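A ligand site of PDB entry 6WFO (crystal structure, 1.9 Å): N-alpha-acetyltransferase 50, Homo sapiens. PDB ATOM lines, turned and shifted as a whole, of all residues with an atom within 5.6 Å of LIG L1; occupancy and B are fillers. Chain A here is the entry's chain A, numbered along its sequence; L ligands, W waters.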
ATOM      1  N   PHE A  29      -2.679 -16.640 -17.407  1.00  0.00           N
ATOM      2  CA  PHE A  29      -1.784 -17.441 -18.219  1.00  0.00           C
ATOM      3  C   PHE A  29      -2.468 -18.632 -18.912  1.00  0.00           C
ATOM      4  O   PHE A  29      -3.395 -19.223 -18.331  1.00  0.00           O
ATOM      5  CB  PHE A  29      -0.554 -17.855 -17.390  1.00  0.00           C
ATOM      6  CG  PHE A  29       0.205 -16.642 -16.888  1.00  0.00           C
ATOM      7  CD1 PHE A  29       0.961 -15.864 -17.761  1.00  0.00           C
ATOM      8  CD2 PHE A  29       0.074 -16.222 -15.557  1.00  0.00           C
ATOM      9  CE1 PHE A  29       1.616 -14.713 -17.307  1.00  0.00           C
ATOM     10  CE2 PHE A  29       0.740 -15.072 -15.113  1.00  0.00           C
ATOM     11  CZ  PHE A  29       1.524 -14.352 -15.983  1.00  0.00           C
ATOM     12  N   PRO A  30      -2.055 -18.988 -20.170  1.00  0.00           N
ATOM     13  CA  PRO A  30      -2.711 -20.128 -20.855  1.00  0.00           C
ATOM     14  C   PRO A  30      -2.219 -21.515 -20.421  1.00  0.00           C
ATOM     15  O   PRO A  30      -2.702 -22.528 -20.945  1.00  0.00           O
ATOM     16  CB  PRO A  30      -2.426 -19.828 -22.330  1.00  0.00           C
ATOM     17  CG  PRO A  30      -1.119 -19.121 -22.324  1.00  0.00           C
ATOM     18  CD  PRO A  30      -1.001 -18.385 -21.011  1.00  0.00           C
ATOM     19  N   VAL A  31      -1.274 -21.560 -19.471  1.00  0.00           N
ATOM     20  CA  VAL A  31      -0.723 -22.784 -18.887  1.00  0.00           C
ATOM     21  C   VAL A  31      -1.051 -22.828 -17.378  1.00  0.00           C
ATOM     22  O   VAL A  31      -1.349 -21.782 -16.776  1.00  0.00           O
ATOM     23  CB  VAL A  31       0.802 -22.997 -19.149  1.00  0.00           C
ATOM     24  CG1 VAL A  31       1.116 -23.016 -20.638  1.00  0.00           C
ATOM     25  CG2 VAL A  31       1.660 -21.960 -18.426  1.00  0.00           C
ATOM     26  N   SER A  32      -1.007 -24.027 -16.784  1.00  0.00           N
ATOM     27  CA  SER A  32      -1.302 -24.259 -15.365  1.00  0.00           C
ATOM     28  C   SER A  32      -0.032 -24.496 -14.585  1.00  0.00           C
ATOM     29  O   SER A  32       0.878 -25.156 -15.085  1.00  0.00           O
ATOM     30  CB  SER A  32      -2.217 -25.468 -15.209  1.00  0.00           C
ATOM     31  OG  SER A  32      -3.414 -25.341 -15.946  1.00  0.00           O
ATOM     32  N   TYR A  33       0.019 -23.990 -13.332  1.00  0.00           N
ATOM     33  CA  TYR A  33       1.163 -24.210 -12.459  1.00  0.00           C
ATOM     34  C   TYR A  33       0.755 -25.110 -11.306  1.00  0.00           C
ATOM     35  O   TYR A  33      -0.407 -25.087 -10.888  1.00  0.00           O
ATOM     36  CB  TYR A  33       1.807 -22.868 -12.028  1.00  0.00           C
ATOM     37  CG  TYR A  33       2.319 -22.075 -13.209  1.00  0.00           C
ATOM     38  CD1 TYR A  33       3.592 -22.318 -13.733  1.00  0.00           C
ATOM     39  CD2 TYR A  33       1.518 -21.136 -13.840  1.00  0.00           C
ATOM     40  CE1 TYR A  33       4.047 -21.620 -14.856  1.00  0.00           C
ATOM     41  CE2 TYR A  33       1.948 -20.460 -14.979  1.00  0.00           C
ATOM     42  CZ  TYR A  33       3.225 -20.696 -15.468  1.00  0.00           C
ATOM     43  OH  TYR A  33       3.662 -20.003 -16.579  1.00  0.00           O
ATOM     44  N   ARG A  64      12.451 -16.697  -9.610  1.00  0.00           N
ATOM     45  CA  ARG A  64      13.329 -17.631  -8.895  1.00  0.00           C
ATOM     46  C   ARG A  64      14.742 -17.390  -9.366  1.00  0.00           C
ATOM     47  O   ARG A  64      14.958 -16.923 -10.496  1.00  0.00           O
ATOM     48  CB  ARG A  64      12.923 -19.116  -9.100  1.00  0.00           C
ATOM     49  CG  ARG A  64      13.139 -19.645 -10.542  1.00  0.00           C
ATOM     50  CD  ARG A  64      12.830 -21.110 -10.747  1.00  0.00           C
ATOM     51  NE  ARG A  64      13.701 -21.990  -9.959  1.00  0.00           N
ATOM     52  CZ  ARG A  64      14.934 -22.348 -10.312  1.00  0.00           C
ATOM     53  NH1 ARG A  64      15.461 -21.930 -11.467  1.00  0.00           N
ATOM     54  NH2 ARG A  64      15.655 -23.131  -9.515  1.00  0.00           N
ATOM     55  N   ASP A  66      18.101 -18.615 -10.725  1.00  0.00           N
ATOM     56  CA  ASP A  66      18.563 -19.684 -11.588  1.00  0.00           C
ATOM     57  C   ASP A  66      20.092 -19.657 -11.711  1.00  0.00           C
ATOM     58  O   ASP A  66      20.665 -18.611 -12.012  1.00  0.00           O
ATOM     59  CB  ASP A  66      17.868 -19.617 -12.978  1.00  0.00           C
ATOM     60  CG  ASP A  66      18.413 -20.576 -14.006  1.00  0.00           C
ATOM     61  OD1 ASP A  66      18.095 -21.779 -13.910  1.00  0.00           O
ATOM     62  OD2 ASP A  66      19.146 -20.133 -14.896  1.00  0.00           O
ATOM     63  N   TYR A  75      15.320 -15.398 -12.970  1.00  0.00           N
ATOM     64  CA  TYR A  75      14.351 -15.918 -13.925  1.00  0.00           C
ATOM     65  C   TYR A  75      12.931 -15.497 -13.560  1.00  0.00           C
ATOM     66  O   TYR A  75      12.441 -15.855 -12.495  1.00  0.00           O
ATOM     67  CB  TYR A  75      14.517 -17.458 -14.111  1.00  0.00           C
ATOM     68  CG  TYR A  75      13.545 -18.061 -15.107  1.00  0.00           C
ATOM     69  CD1 TYR A  75      13.710 -17.842 -16.489  1.00  0.00           C
ATOM     70  CD2 TYR A  75      12.480 -18.849 -14.687  1.00  0.00           C
ATOM     71  CE1 TYR A  75      12.804 -18.386 -17.406  1.00  0.00           C
ATOM     72  CE2 TYR A  75      11.551 -19.358 -15.600  1.00  0.00           C
ATOM     73  CZ  TYR A  75      11.738 -19.127 -16.958  1.00  0.00           C
ATOM     74  OH  TYR A  75      10.821 -19.596 -17.860  1.00  0.00           O
ATOM     75  N   ILE A  76      12.262 -14.741 -14.478  1.00  0.00           N
ATOM     76  CA  ILE A  76      10.878 -14.321 -14.324  1.00  0.00           C
ATOM     77  C   ILE A  76       9.992 -15.416 -14.865  1.00  0.00           C
ATOM     78  O   ILE A  76       9.976 -15.667 -16.073  1.00  0.00           O
ATOM     79  CB  ILE A  76      10.527 -12.924 -14.920  1.00  0.00           C
ATOM     80  CG1 ILE A  76      11.490 -11.808 -14.411  1.00  0.00           C
ATOM     81  CG2 ILE A  76       9.041 -12.550 -14.656  1.00  0.00           C
ATOM     82  CD1 ILE A  76      11.402 -10.516 -15.237  1.00  0.00           C
ATOM     83  N   MET A  77       9.217 -16.049 -13.970  1.00  0.00           N
ATOM     84  CA  MET A  77       8.340 -17.168 -14.331  1.00  0.00           C
ATOM     85  C   MET A  77       7.011 -16.721 -14.863  1.00  0.00           C
ATOM     86  O   MET A  77       6.539 -17.227 -15.864  1.00  0.00           O
ATOM     87  CB  MET A  77       8.185 -18.074 -13.111  1.00  0.00           C
ATOM     88  CG  MET A  77       9.521 -18.421 -12.524  1.00  0.00           C
ATOM     89  SD  MET A  77       9.410 -19.608 -11.199  1.00  0.00           S
ATOM     90  CE  MET A  77       8.889 -21.128 -12.146  1.00  0.00           C
ATOM     91  N   THR A  78       6.362 -15.836 -14.122  1.00  0.00           N
ATOM     92  CA  THR A  78       5.060 -15.262 -14.432  1.00  0.00           C
ATOM     93  C   THR A  78       5.115 -13.808 -14.032  1.00  0.00           C
ATOM     94  O   THR A  78       5.685 -13.472 -12.999  1.00  0.00           O
ATOM     95  CB  THR A  78       3.941 -15.980 -13.624  1.00  0.00           C
ATOM     96  OG1 THR A  78       4.287 -15.969 -12.231  1.00  0.00           O
ATOM     97  CG2 THR A  78       3.660 -17.401 -14.105  1.00  0.00           C
ATOM     98  N   TYR A 112      16.242 -13.097 -17.252  1.00  0.00           N
ATOM     99  CA  TYR A 112      15.624 -13.684 -18.428  1.00  0.00           C
ATOM    100  C   TYR A 112      14.250 -14.276 -18.125  1.00  0.00           C
ATOM    101  O   TYR A 112      13.858 -14.380 -16.956  1.00  0.00           O
ATOM    102  CB  TYR A 112      16.574 -14.696 -19.096  1.00  0.00           C
ATOM    103  CG  TYR A 112      16.647 -16.068 -18.461  1.00  0.00           C
ATOM    104  CD1 TYR A 112      17.304 -16.266 -17.240  1.00  0.00           C
ATOM    105  CD2 TYR A 112      16.144 -17.188 -19.115  1.00  0.00           C
ATOM    106  CE1 TYR A 112      17.415 -17.537 -16.673  1.00  0.00           C
ATOM    107  CE2 TYR A 112      16.260 -18.470 -18.564  1.00  0.00           C
ATOM    108  CZ  TYR A 112      16.907 -18.639 -17.356  1.00  0.00           C
ATOM    109  OH  TYR A 112      17.044 -19.906 -16.824  1.00  0.00           O
ATOM    110  N   HIS A 114      10.782 -16.578 -20.653  1.00  0.00           N
ATOM    111  CA  HIS A 114      10.298 -17.153 -21.903  1.00  0.00           C
ATOM    112  C   HIS A 114       8.985 -16.482 -22.241  1.00  0.00           C
ATOM    113  O   HIS A 114       8.201 -16.166 -21.313  1.00  0.00           O
ATOM    114  CB  HIS A 114      10.120 -18.665 -21.795  1.00  0.00           C
ATOM    115  CG  HIS A 114      11.413 -19.412 -21.705  1.00  0.00           C
ATOM    116  ND1 HIS A 114      11.980 -19.712 -20.484  1.00  0.00           N
ATOM    117  CD2 HIS A 114      12.199 -19.898 -22.696  1.00  0.00           C
ATOM    118  CE1 HIS A 114      13.105 -20.372 -20.750  1.00  0.00           C
ATOM    119  NE2 HIS A 114      13.276 -20.521 -22.074  1.00  0.00           N
ATOM    120  N   VAL A 115       8.745 -16.215 -23.533  1.00  0.00           N
ATOM    121  CA  VAL A 115       7.515 -15.573 -24.020  1.00  0.00           C
ATOM    122  C   VAL A 115       7.070 -16.385 -25.215  1.00  0.00           C
ATOM    123  O   VAL A 115       7.819 -16.447 -26.185  1.00  0.00           O
ATOM    124  CB  VAL A 115       7.716 -14.082 -24.458  1.00  0.00           C
ATOM    125  CG1 VAL A 115       6.385 -13.434 -24.835  1.00  0.00           C
ATOM    126  CG2 VAL A 115       8.444 -13.246 -23.405  1.00  0.00           C
ATOM    127  N   GLN A 116       5.821 -16.913 -25.188  1.00  0.00           N
ATOM    128  CA  GLN A 116       5.187 -17.568 -26.315  1.00  0.00           C
ATOM    129  C   GLN A 116       5.239 -16.566 -27.485  1.00  0.00           C
ATOM    130  O   GLN A 116       4.797 -15.430 -27.338  1.00  0.00           O
ATOM    131  CB  GLN A 116       3.734 -17.879 -25.957  1.00  0.00           C
ATOM    132  CG  GLN A 116       3.088 -18.949 -26.813  1.00  0.00           C
ATOM    133  CD  GLN A 116       1.682 -19.300 -26.369  1.00  0.00           C
ATOM    134  OE1 GLN A 116       1.092 -18.694 -25.454  1.00  0.00           O
ATOM    135  NE2 GLN A 116       1.092 -20.290 -27.022  1.00  0.00           N
ATOM    136  N   ASN A 119       2.809 -13.762 -28.445  1.00  0.00           N
ATOM    137  CA  ASN A 119       2.565 -12.673 -27.494  1.00  0.00           C
ATOM    138  C   ASN A 119       3.356 -11.386 -27.841  1.00  0.00           C
ATOM    139  O   ASN A 119       4.373 -11.078 -27.241  1.00  0.00           O
ATOM    140  CB  ASN A 119       2.867 -13.169 -26.080  1.00  0.00           C
ATOM    141  CG  ASN A 119       2.163 -12.423 -24.983  1.00  0.00           C
ATOM    142  OD1 ASN A 119       1.737 -11.284 -25.122  1.00  0.00           O
ATOM    143  ND2 ASN A 119       2.049 -13.078 -23.857  1.00  0.00           N
ATOM    144  N   TYR A 140       8.622 -25.425 -26.937  1.00  0.00           N
ATOM    145  CA  TYR A 140       8.835 -25.156 -25.526  1.00  0.00           C
ATOM    146  C   TYR A 140       7.545 -25.554 -24.775  1.00  0.00           C
ATOM    147  O   TYR A 140       7.638 -26.246 -23.766  1.00  0.00           O
ATOM    148  CB  TYR A 140       9.192 -23.675 -25.332  1.00  0.00           C
ATOM    149  CG  TYR A 140       9.475 -23.286 -23.903  1.00  0.00           C
ATOM    150  CD1 TYR A 140      10.723 -23.511 -23.335  1.00  0.00           C
ATOM    151  CD2 TYR A 140       8.521 -22.646 -23.125  1.00  0.00           C
ATOM    152  CE1 TYR A 140      10.994 -23.142 -22.012  1.00  0.00           C
ATOM    153  CE2 TYR A 140       8.762 -22.288 -21.802  1.00  0.00           C
ATOM    154  CZ  TYR A 140      10.010 -22.536 -21.255  1.00  0.00           C
ATOM    155  OH  TYR A 140      10.267 -22.139 -19.959  1.00  0.00           O
ATOM    156  N   TYR A 141       6.362 -25.167 -25.280  1.00  0.00           N
ATOM    157  CA  TYR A 141       5.081 -25.511 -24.648  1.00  0.00           C
ATOM    158  C   TYR A 141       4.531 -26.846 -25.186  1.00  0.00           C
ATOM    159  O   TYR A 141       4.457 -27.049 -26.397  1.00  0.00           O
ATOM    160  CB  TYR A 141       4.055 -24.361 -24.741  1.00  0.00           C
ATOM    161  CG  TYR A 141       4.604 -23.060 -24.202  1.00  0.00           C
ATOM    162  CD1 TYR A 141       4.731 -22.842 -22.829  1.00  0.00           C
ATOM    163  CD2 TYR A 141       5.035 -22.054 -25.065  1.00  0.00           C
ATOM    164  CE1 TYR A 141       5.255 -21.647 -22.333  1.00  0.00           C
ATOM    165  CE2 TYR A 141       5.553 -20.853 -24.575  1.00  0.00           C
ATOM    166  CZ  TYR A 141       5.684 -20.664 -23.217  1.00  0.00           C
ATOM    167  OH  TYR A 141       6.274 -19.528 -22.719  1.00  0.00           O
ATOM    168  N   LYS A 142       4.167 -27.731 -24.268  1.00  0.00           N
ATOM    169  CA  LYS A 142       3.706 -29.079 -24.572  1.00  0.00           C
ATOM    170  C   LYS A 142       2.314 -29.187 -25.195  1.00  0.00           C
ATOM    171  O   LYS A 142       2.164 -29.903 -26.168  1.00  0.00           O
ATOM    172  CB  LYS A 142       3.806 -29.967 -23.315  1.00  0.00           C
ATOM    173  CG  LYS A 142       5.226 -30.151 -22.794  1.00  0.00           C
ATOM    174  N   ARG A 143       1.294 -28.522 -24.627  1.00  0.00           N
ATOM    175  CA  ARG A 143      -0.093 -28.672 -25.084  1.00  0.00           C
ATOM    176  C   ARG A 143      -0.777 -27.398 -25.618  1.00  0.00           C
ATOM    177  O   ARG A 143      -1.994 -27.431 -25.854  1.00  0.00           O
ATOM    178  CB  ARG A 143      -0.934 -29.309 -23.956  1.00  0.00           C
ATOM    179  N   ILE A 144      -0.022 -26.302 -25.837  1.00  0.00           N
ATOM    180  CA  ILE A 144      -0.643 -25.058 -26.341  1.00  0.00           C
ATOM    181  C   ILE A 144      -0.006 -24.583 -27.652  1.00  0.00           C
ATOM    182  O   ILE A 144       1.173 -24.828 -27.902  1.00  0.00           O
ATOM    183  CB  ILE A 144      -0.703 -23.907 -25.265  1.00  0.00           C
ATOM    184  CG1 ILE A 144       0.683 -23.287 -24.970  1.00  0.00           C
ATOM    185  CG2 ILE A 144      -1.407 -24.380 -23.976  1.00  0.00           C
ATOM    186  CD1 ILE A 144       0.696 -22.024 -24.145  1.00  0.00           C
HETATM  187  C1  LIG L   1       4.964 -25.334 -19.844  1.00  0.00           C
HETATM  188  C2  LIG L   1       3.191 -25.447 -18.180  1.00  0.00           C
HETATM  189  C3  LIG L   1       5.841 -24.805 -18.883  1.00  0.00           C
HETATM  190  C4  LIG L   1       4.067 -24.912 -17.212  1.00  0.00           C
HETATM  191  C5  LIG L   1      11.606 -23.434 -16.774  1.00  0.00           C
HETATM  192  C6  LIG L   1       3.644 -25.661 -19.486  1.00  0.00           C
HETATM  193  C7  LIG L   1       5.375 -24.591 -17.582  1.00  0.00           C
HETATM  194  C8  LIG L   1      11.596 -22.767 -15.575  1.00  0.00           C
HETATM  195  C9  LIG L   1       2.721 -26.202 -20.515  1.00  0.00           C
HETATM  196  C10 LIG L   1       9.415 -22.676 -15.991  1.00  0.00           C
HETATM  197  C11 LIG L   1       3.411 -18.167 -19.235  1.00  0.00           C
HETATM  198  C12 LIG L   1       4.603 -17.286 -21.250  1.00  0.00           C
HETATM  199  C13 LIG L   1       6.271 -24.050 -16.560  1.00  0.00           C
HETATM  200  C14 LIG L   1      12.799 -22.477 -14.813  1.00  0.00           C
HETATM  201  C15 LIG L   1       6.468 -18.962 -19.072  1.00  0.00           C
HETATM  202  C16 LIG L   1       4.534 -17.510 -18.434  1.00  0.00           C
HETATM  203  C17 LIG L   1       7.774 -20.799 -16.071  1.00  0.00           C
HETATM  204  C18 LIG L   1       6.501 -21.823 -17.781  1.00  0.00           C
HETATM  205  C19 LIG L   1       7.938 -22.312 -15.873  1.00  0.00           C
HETATM  206  C20 LIG L   1       5.885 -17.580 -19.124  1.00  0.00           C
HETATM  207  C21 LIG L   1       7.469 -20.652 -17.564  1.00  0.00           C
HETATM  208  C22 LIG L   1       2.652 -18.740 -21.540  1.00  0.00           C
HETATM  209  N1  LIG L   1       3.079 -26.482 -21.785  1.00  0.00           N
HETATM  210  N2  LIG L   1      10.351 -22.342 -15.134  1.00  0.00           N
HETATM  211  N3  LIG L   1       1.398 -26.394 -20.304  1.00  0.00           N
HETATM  212  N4  LIG L   1       1.927 -26.861 -22.383  1.00  0.00           N
HETATM  213  N5  LIG L   1       0.915 -26.823 -21.499  1.00  0.00           N
HETATM  214  N6  LIG L   1       5.773 -17.192 -20.512  1.00  0.00           N
HETATM  215  N7  LIG L   1       3.612 -18.099 -20.643  1.00  0.00           N
HETATM  216  N8  LIG L   1       6.980 -22.880 -16.866  1.00  0.00           N
HETATM  217  N9  LIG L   1       6.932 -19.323 -17.835  1.00  0.00           N
HETATM  218  O1  LIG L   1       2.451 -18.659 -18.664  1.00  0.00           O
HETATM  219  O2  LIG L   1       4.448 -16.744 -22.328  1.00  0.00           O
HETATM  220  O3  LIG L   1       6.324 -24.688 -15.515  1.00  0.00           O
HETATM  221  O4  LIG L   1      13.770 -21.873 -15.273  1.00  0.00           O
HETATM  222  O5  LIG L   1       6.523 -19.706 -20.040  1.00  0.00           O
HETATM  223  S1  LIG L   1       9.997 -23.530 -17.341  1.00  0.00           S
HETATM  224  N1  LG2 L   2       1.147  -2.934 -27.150  1.00  0.00           N
HETATM  225  C1  LG2 L   2       2.259  -2.203 -27.275  1.00  0.00           C
HETATM  226  N2  LG2 L   2       3.130  -1.830 -26.324  1.00  0.00           N
HETATM  227  C2  LG2 L   2       2.774  -2.321 -25.126  1.00  0.00           C
HETATM  228  C3  LG2 L   2       1.672  -3.106 -24.851  1.00  0.00           C
HETATM  229  C4  LG2 L   2       0.818  -3.419 -25.922  1.00  0.00           C
HETATM  230  N3  LG2 L   2      -0.307  -4.132 -25.802  1.00  0.00           N
HETATM  231  N4  LG2 L   2       1.634  -3.433 -23.502  1.00  0.00           N
HETATM  232  C5  LG2 L   2       2.696  -2.846 -23.004  1.00  0.00           C
HETATM  233  N5  LG2 L   2       3.412  -2.131 -23.917  1.00  0.00           N
HETATM  234  C6  LG2 L   2       4.552  -1.252 -23.653  1.00  0.00           C
HETATM  235  C7  LG2 L   2       4.230   0.241 -23.844  1.00  0.00           C
HETATM  236  O1  LG2 L   2       5.312   0.979 -24.390  1.00  0.00           O
HETATM  237  C8  LG2 L   2       3.865   0.624 -22.409  1.00  0.00           C
HETATM  238  O2  LG2 L   2       4.001   2.037 -22.150  1.00  0.00           O
HETATM  239  P1  LG2 L   2       2.747   3.033 -22.399  1.00  0.00           P
HETATM  240  O3  LG2 L   2       3.023   4.299 -21.654  1.00  0.00           O
HETATM  241  O4  LG2 L   2       2.678   3.207 -23.960  1.00  0.00           O
HETATM  242  O5  LG2 L   2       1.478   2.275 -21.920  1.00  0.00           O
HETATM  243  C9  LG2 L   2       4.860  -0.171 -21.585  1.00  0.00           C
HETATM  244  O6  LG2 L   2       4.954  -1.429 -22.304  1.00  0.00           O
HETATM  245  C10 LG2 L   2       4.498  -0.424 -20.144  1.00  0.00           C
HETATM  246  O7  LG2 L   2       3.179  -1.030 -20.063  1.00  0.00           O
HETATM  247  P2  LG2 L   2       2.366  -1.261 -18.697  1.00  0.00           P
HETATM  248  O8  LG2 L   2       1.216  -0.380 -18.575  1.00  0.00           O
HETATM  249  O9  LG2 L   2       3.225  -1.210 -17.469  1.00  0.00           O
HETATM  250  O10 LG2 L   2       1.918  -2.776 -18.957  1.00  0.00           O
HETATM  251  P3  LG2 L   2       0.859  -3.845 -18.431  1.00  0.00           P
HETATM  252  O11 LG2 L   2       0.379  -3.485 -17.078  1.00  0.00           O
HETATM  253  O12 LG2 L   2      -0.291  -3.812 -19.393  1.00  0.00           O
HETATM  254  O13 LG2 L   2       1.755  -5.144 -18.429  1.00  0.00           O
HETATM  255  C11 LG2 L   2       1.880  -7.296 -19.716  1.00  0.00           C
HETATM  256  C12 LG2 L   2       2.102  -5.781 -19.681  1.00  0.00           C
HETATM  257  C13 LG2 L   2       2.440  -7.923 -18.422  1.00  0.00           C
HETATM  258  C14 LG2 L   2       2.639  -7.884 -20.908  1.00  0.00           C
HETATM  259  C15 LG2 L   2       0.346  -7.537 -19.805  1.00  0.00           C
HETATM  260  O14 LG2 L   2      -0.145  -7.171 -21.094  1.00  0.00           O
HETATM  261  C16 LG2 L   2      -0.190  -8.906 -19.447  1.00  0.00           C
HETATM  262  O15 LG2 L   2      -0.646  -9.113 -18.320  1.00  0.00           O
HETATM  263  N6  LG2 L   2      -0.231  -9.821 -20.426  1.00  0.00           N
HETATM  264  C17 LG2 L   2      -0.668 -11.191 -20.221  1.00  0.00           C
HETATM  265  C18 LG2 L   2       0.399 -12.021 -19.556  1.00  0.00           C
HETATM  266  C19 LG2 L   2       1.736 -11.830 -20.234  1.00  0.00           C
HETATM  267  O16 LG2 L   2       1.825 -11.807 -21.457  1.00  0.00           O
HETATM  268  N7  LG2 L   2       2.791 -11.709 -19.435  1.00  0.00           N
HETATM  269  C20 LG2 L   2       4.147 -11.912 -19.913  1.00  0.00           C
HETATM  270  C21 LG2 L   2       4.355 -13.366 -20.299  1.00  0.00           C
HETATM  271  S1  LG2 L   2       6.075 -13.749 -20.014  1.00  0.00           S
HETATM  272  C22 LG2 L   2       6.090 -13.939 -18.260  1.00  0.00           C
HETATM  273  O17 LG2 L   2       5.082 -13.989 -17.607  1.00  0.00           O
HETATM  274  C23 LG2 L   2       7.463 -14.191 -17.712  1.00  0.00           C
HETATM  275  O   HOH W   1       2.271 -15.859 -23.725  1.00  0.00           O
HETATM  276  O   HOH W   2      -1.165 -26.410 -18.575  1.00  0.00           O
HETATM  277  O   HOH W   3       9.535 -17.221 -18.240  1.00  0.00           O
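A ring nitrogen (ND1) of His 114 sits at hydrogen-bond distance from the side-chain hydroxyl of Tyr 140, at 3.0 Å. A ring nitrogen (ND1) of His 114 is in hydrogen-bond range of the side-chain hydroxyl (OH) of Tyr 75. The side-chain hydroxyl (OH) of Tyr 140 is in hydrogen-bond range of the side-chain hydroxyl (OH) of Tyr 75, at 3.3 Å. O of Arg 64 lies within hydrogen-bond range of N of Tyr 75 (2.9 Å).
O5 of LIG L1 lies within hydrogen-bond range of OH of Tyr 141 (2.7 Å). The backbone carbonyl oxygen (O) of His 114 is in hydrogen-bond range of a nitrogen (N6) of LIG L1 (2.8 Å). An oxygen (O1) of LIG L1 sits at hydrogen-bond distance from the side-chain hydroxyl of Tyr 33, 2.8 Å away. The backbone NH of Arg 143 lies within hydrogen-bond range of a nitrogen (N4) of LIG L1 (2.9 Å). O of Met 77 is in hydrogen-bond range of N9 of LIG L1 (2.9 Å). The side-chain hydroxyl of Tyr 140 sits close to a sulfur (S1) of LIG L1, 3.0 Å away. The backbone NH of Lys 142 lies within hydrogen-bond range of a nitrogen (N1) of LIG L1. N of Gln 116 is in hydrogen-bond range of O2 of LIG L1, at 3.2 Å. O16 of LG2 L2 is in hydrogen-bond range of ND2 of Asn 119 (2.7 Å).
A nitrogen (N6) of LIG L1 sits close to a sulfur (S1) of LG2 L2 (3.5 Å).
Water W1 bridges an oxygen (O2) of LIG L1 (2.7 Å) and the side-chain amide nitrogen of Asn 119 (2.8 Å). Water W2 lies within hydrogen-bond range of the backbone NH (N) of Ser 32 (3.0 Å) and a nitrogen (N3) of LIG L1 (3.1 Å). Water W3 lies within hydrogen-bond range of the backbone carbonyl oxygen (O) of Ile 76 (2.7 Å), the side-chain hydroxyl (OH) of Tyr 75 (2.7 Å), the backbone NH (N) of His 114 (2.8 Å) and a nitrogen (N9) of LIG L1 (3.4 Å).
Phe 29 touches LIG L1 (CD1 to O1, 3.3 Å). Pro 30 touches LIG L1 (CD to C22, 3.7 Å). Val 31 touches LIG L1 (CG2 to O1, 3.4 Å). O of Ser 32 touches C4 of LIG L1, 3.8 Å away. CE2 of Tyr 75 touches N2 of LIG L1, 3.2 Å away. CA of Val 115 touches O2 of LIG L1, 3.7 Å away. The nearest printed residue that does not touch LIG L1 is Ile 144 (4.01 Å).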
